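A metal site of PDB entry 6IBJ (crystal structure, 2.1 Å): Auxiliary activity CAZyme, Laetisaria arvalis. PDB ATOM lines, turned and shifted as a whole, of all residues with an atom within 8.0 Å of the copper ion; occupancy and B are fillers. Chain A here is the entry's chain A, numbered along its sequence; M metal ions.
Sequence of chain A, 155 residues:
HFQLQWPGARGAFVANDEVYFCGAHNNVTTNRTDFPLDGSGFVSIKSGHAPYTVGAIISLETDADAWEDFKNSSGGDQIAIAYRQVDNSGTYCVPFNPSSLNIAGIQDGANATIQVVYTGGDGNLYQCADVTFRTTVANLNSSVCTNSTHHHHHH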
ATOM      1  N   HIS A   1      22.474  10.660  30.349  1.00  0.00           N
ATOM      2  CA  HIS A   1      23.480  10.818  29.212  1.00  0.00           C
ATOM      3  C   HIS A   1      22.781  10.633  27.861  1.00  0.00           C
ATOM      4  O   HIS A   1      21.678  10.077  27.791  1.00  0.00           O
ATOM      5  CB  HIS A   1      24.657   9.871  29.456  1.00  0.00           C
ATOM      6  CG  HIS A   1      25.505  10.334  30.591  1.00  0.00           C
ATOM      7  ND1 HIS A   1      24.978  10.637  31.848  1.00  0.00           N
ATOM      8  CD2 HIS A   1      26.823  10.634  30.643  1.00  0.00           C
ATOM      9  CE1 HIS A   1      25.956  11.081  32.631  1.00  0.00           C
ATOM     10  NE2 HIS A   1      27.099  11.070  31.911  1.00  0.00           N
ATOM     11  N   PHE A   2      23.414  11.107  26.771  1.00  0.00           N
ATOM     12  CA  PHE A   2      22.801  11.019  25.454  1.00  0.00           C
ATOM     13  C   PHE A   2      23.845  10.777  24.347  1.00  0.00           C
ATOM     14  O   PHE A   2      25.023  11.097  24.453  1.00  0.00           O
ATOM     15  CB  PHE A   2      22.001  12.293  25.165  1.00  0.00           C
ATOM     16  CG  PHE A   2      22.868  13.476  24.793  1.00  0.00           C
ATOM     17  CD1 PHE A   2      23.566  14.184  25.769  1.00  0.00           C
ATOM     18  CD2 PHE A   2      23.012  13.867  23.467  1.00  0.00           C
ATOM     19  CE1 PHE A   2      24.355  15.272  25.416  1.00  0.00           C
ATOM     20  CE2 PHE A   2      23.810  14.959  23.119  1.00  0.00           C
ATOM     21  CZ  PHE A   2      24.494  15.643  24.095  1.00  0.00           C
ATOM     22  N   GLN A   3      23.368  10.248  23.229  1.00  0.00           N
ATOM     23  CA  GLN A   3      24.165  10.062  22.026  1.00  0.00           C
ATOM     24  C   GLN A   3      23.391  10.721  20.869  1.00  0.00           C
ATOM     25  O   GLN A   3      22.175  10.607  20.771  1.00  0.00           O
ATOM     26  CB  GLN A   3      24.449   8.579  21.776  1.00  0.00           C
ATOM     27  CG  GLN A   3      24.917   7.805  23.002  1.00  0.00           C
ATOM     28  CD  GLN A   3      23.826   7.045  23.757  1.00  0.00           C
ATOM     29  OE1 GLN A   3      23.126   6.203  23.187  1.00  0.00           O
ATOM     30  NE2 GLN A   3      23.699   7.298  25.057  1.00  0.00           N
ATOM     31  N   PHE A  13      31.162   8.161  21.452  1.00  0.00           N
ATOM     32  CA  PHE A  13      30.514   8.449  22.726  1.00  0.00           C
ATOM     33  C   PHE A  13      31.305   7.822  23.871  1.00  0.00           C
ATOM     34  O   PHE A  13      31.412   6.609  23.936  1.00  0.00           O
ATOM     35  CB  PHE A  13      29.079   7.922  22.711  1.00  0.00           C
ATOM     36  CG  PHE A  13      28.438   7.859  24.065  1.00  0.00           C
ATOM     37  CD1 PHE A  13      27.840   8.977  24.629  1.00  0.00           C
ATOM     38  CD2 PHE A  13      28.415   6.660  24.775  1.00  0.00           C
ATOM     39  CE1 PHE A  13      27.242   8.900  25.880  1.00  0.00           C
ATOM     40  CE2 PHE A  13      27.836   6.604  26.043  1.00  0.00           C
ATOM     41  CZ  PHE A  13      27.249   7.717  26.591  1.00  0.00           C
ATOM     42  N   ALA A  15      30.757   8.282  27.920  1.00  0.00           N
ATOM     43  CA  ALA A  15      29.830   8.800  28.925  1.00  0.00           C
ATOM     44  C   ALA A  15      30.517   9.838  29.850  1.00  0.00           C
ATOM     45  O   ALA A  15      30.028  10.960  29.969  1.00  0.00           O
ATOM     46  CB  ALA A  15      29.242   7.636  29.680  1.00  0.00           C
ATOM     47  N   GLU A  18      31.358  13.511  28.397  1.00  0.00           N
ATOM     48  CA  GLU A  18      30.279  14.423  27.956  1.00  0.00           C
ATOM     49  C   GLU A  18      30.241  15.715  28.782  1.00  0.00           C
ATOM     50  O   GLU A  18      29.671  16.727  28.352  1.00  0.00           O
ATOM     51  CB  GLU A  18      28.909  13.738  27.983  1.00  0.00           C
ATOM     52  CG  GLU A  18      28.736  12.753  26.857  1.00  0.00           C
ATOM     53  CD  GLU A  18      27.308  12.306  26.566  1.00  0.00           C
ATOM     54  OE1 GLU A  18      26.474  12.250  27.508  1.00  0.00           O
ATOM     55  OE2 GLU A  18      27.043  12.033  25.386  1.00  0.00           O
ATOM     56  N   SER A  47      18.473   9.385  24.793  1.00  0.00           N
ATOM     57  CA  SER A  47      18.784   9.629  26.241  1.00  0.00           C
ATOM     58  C   SER A  47      18.480   8.381  27.087  1.00  0.00           C
ATOM     59  O   SER A  47      17.472   7.759  26.902  1.00  0.00           O
ATOM     60  CB  SER A  47      18.009  10.796  26.791  1.00  0.00           C
ATOM     61  OG  SER A  47      18.309  10.984  28.165  1.00  0.00           O
ATOM     62  N   GLY A  48      19.346   8.062  28.045  1.00  0.00           N
ATOM     63  CA  GLY A  48      19.144   6.926  28.905  1.00  0.00           C
ATOM     64  C   GLY A  48      18.169   7.210  30.054  1.00  0.00           C
ATOM     65  O   GLY A  48      17.764   6.285  30.746  1.00  0.00           O
ATOM     66  N   HIS A  49      17.817   8.473  30.285  1.00  0.00           N
ATOM     67  CA  HIS A  49      16.887   8.814  31.368  1.00  0.00           C
ATOM     68  C   HIS A  49      16.175  10.128  31.083  1.00  0.00           C
ATOM     69  O   HIS A  49      16.618  10.921  30.250  1.00  0.00           O
ATOM     70  CB  HIS A  49      17.615   8.871  32.718  1.00  0.00           C
ATOM     71  CG  HIS A  49      18.899   9.627  32.712  1.00  0.00           C
ATOM     72  ND1 HIS A  49      18.953  10.981  32.980  1.00  0.00           N
ATOM     73  CD2 HIS A  49      20.176   9.212  32.507  1.00  0.00           C
ATOM     74  CE1 HIS A  49      20.227  11.371  32.976  1.00  0.00           C
ATOM     75  NE2 HIS A  49      21.000  10.315  32.657  1.00  0.00           N
ATOM     76  N   ALA A  50      15.049  10.316  31.794  1.00  0.00           N
ATOM     77  CA  ALA A  50      14.221  11.497  31.736  1.00  0.00           C
ATOM     78  C   ALA A  50      13.664  11.766  33.131  1.00  0.00           C
ATOM     79  O   ALA A  50      13.531  10.844  33.917  1.00  0.00           O
ATOM     80  CB  ALA A  50      13.122  11.307  30.725  1.00  0.00           C
ATOM     81  N   TYR A  52      14.838  15.553  31.262  1.00  0.00           N
ATOM     82  CA  TYR A  52      16.024  16.317  31.037  1.00  0.00           C
ATOM     83  C   TYR A  52      15.660  17.560  30.235  1.00  0.00           C
ATOM     84  O   TYR A  52      14.610  17.629  29.595  1.00  0.00           O
ATOM     85  CB  TYR A  52      17.061  15.452  30.307  1.00  0.00           C
ATOM     86  CG  TYR A  52      16.664  14.979  28.929  1.00  0.00           C
ATOM     87  CD1 TYR A  52      16.932  15.736  27.806  1.00  0.00           C
ATOM     88  CD2 TYR A  52      16.071  13.735  28.735  1.00  0.00           C
ATOM     89  CE1 TYR A  52      16.603  15.289  26.534  1.00  0.00           C
ATOM     90  CE2 TYR A  52      15.733  13.269  27.476  1.00  0.00           C
ATOM     91  CZ  TYR A  52      16.004  14.055  26.369  1.00  0.00           C
ATOM     92  OH  TYR A  52      15.679  13.615  25.109  1.00  0.00           O
ATOM     93  N   TYR A 118      22.804  19.461  27.196  1.00  0.00           N
ATOM     94  CA  TYR A 118      21.913  18.552  27.879  1.00  0.00           C
ATOM     95  C   TYR A 118      22.176  18.669  29.387  1.00  0.00           C
ATOM     96  O   TYR A 118      23.321  18.728  29.823  1.00  0.00           O
ATOM     97  CB  TYR A 118      22.142  17.144  27.340  1.00  0.00           C
ATOM     98  CG  TYR A 118      21.484  15.963  28.034  1.00  0.00           C
ATOM     99  CD1 TYR A 118      21.936  15.495  29.261  1.00  0.00           C
ATOM    100  CD2 TYR A 118      20.512  15.214  27.389  1.00  0.00           C
ATOM    101  CE1 TYR A 118      21.410  14.364  29.861  1.00  0.00           C
ATOM    102  CE2 TYR A 118      19.953  14.085  27.980  1.00  0.00           C
ATOM    103  CZ  TYR A 118      20.424  13.640  29.200  1.00  0.00           C
ATOM    104  OH  TYR A 118      19.928  12.516  29.779  1.00  0.00           O
ATOM    105  N   THR A 119      21.088  18.682  30.163  1.00  0.00           N
ATOM    106  CA  THR A 119      21.183  18.496  31.605  1.00  0.00           C
ATOM    107  C   THR A 119      20.001  17.637  32.070  1.00  0.00           C
ATOM    108  O   THR A 119      18.842  18.026  31.882  1.00  0.00           O
ATOM    109  CB  THR A 119      21.361  19.848  32.301  1.00  0.00           C
ATOM    110  OG1 THR A 119      21.623  19.500  33.654  1.00  0.00           O
ATOM    111  CG2 THR A 119      20.169  20.761  32.216  1.00  0.00           C
ATOM    112  N   GLY A 120      20.320  16.463  32.616  1.00  0.00           N
ATOM    113  CA  GLY A 120      19.328  15.459  33.074  1.00  0.00           C
ATOM    114  C   GLY A 120      19.592  14.980  34.506  1.00  0.00           C
ATOM    115  O   GLY A 120      19.170  13.900  34.873  1.00  0.00           O
ATOM    116  N   GLY A 121      20.295  15.785  35.296  1.00  0.00           N
ATOM    117  CA  GLY A 121      20.513  15.524  36.715  1.00  0.00           C
ATOM    118  C   GLY A 121      21.901  14.984  37.043  1.00  0.00           C
ATOM    119  O   GLY A 121      22.253  14.839  38.239  1.00  0.00           O
ATOM    120  N   ASP A 122      22.715  14.730  36.006  1.00  0.00           N
ATOM    121  CA  ASP A 122      24.082  14.131  36.182  1.00  0.00           C
ATOM    122  C   ASP A 122      25.110  14.910  35.345  1.00  0.00           C
ATOM    123  O   ASP A 122      25.872  14.326  34.589  1.00  0.00           O
ATOM    124  CB  ASP A 122      24.083  12.627  35.850  1.00  0.00           C
ATOM    125  CG  ASP A 122      23.495  12.251  34.495  1.00  0.00           C
ATOM    126  OD1 ASP A 122      22.935  13.132  33.810  1.00  0.00           O
ATOM    127  OD2 ASP A 122      23.630  11.078  34.103  1.00  0.00           O
ATOM    128  N   GLY A 123      25.111  16.230  35.506  1.00  0.00           N
ATOM    129  CA  GLY A 123      26.028  17.091  34.855  1.00  0.00           C
ATOM    130  C   GLY A 123      25.387  17.871  33.715  1.00  0.00           C
ATOM    131  O   GLY A 123      24.271  17.530  33.204  1.00  0.00           O
ATOM    132  N   LEU A 125      26.101  18.258  29.970  1.00  0.00           N
ATOM    133  CA  LEU A 125      26.662  17.311  29.025  1.00  0.00           C
ATOM    134  C   LEU A 125      26.582  17.851  27.601  1.00  0.00           C
ATOM    135  O   LEU A 125      25.658  18.588  27.250  1.00  0.00           O
ATOM    136  CB  LEU A 125      25.896  15.995  29.149  1.00  0.00           C
ATOM    137  CG  LEU A 125      25.806  15.459  30.578  1.00  0.00           C
ATOM    138  CD1 LEU A 125      25.081  14.123  30.612  1.00  0.00           C
ATOM    139  CD2 LEU A 125      27.191  15.328  31.210  1.00  0.00           C
HETATM  140 CU    CU M   1      22.990  10.543  32.305  1.00  0.00          CU
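The backbone NH (N) of His 1 lies close to the side-chain hydroxyl (OH) of Tyr 118 (3.2 Å).
The backbone carbonyl oxygen (O) of His 1 sits at hydrogen-bond distance from the backbone NH (N) of Gly 48.
O of Gly 120 sits close to ND1 of His 49, 3.5 Å away.
The backbone carbonyl oxygen (O) of His 49 lies within hydrogen-bond range of the side-chain hydroxyl (OG) of Ser 47 (2.7 Å).
Within 4 Å of the copper ion: His 1, His 49 and Asp 122.
The copper ion is bound by OD2 of Asp 122, N of His 1, NE2 of His 49 and ND1 of His 1.
The copper ion has four donor atoms within binding distance.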
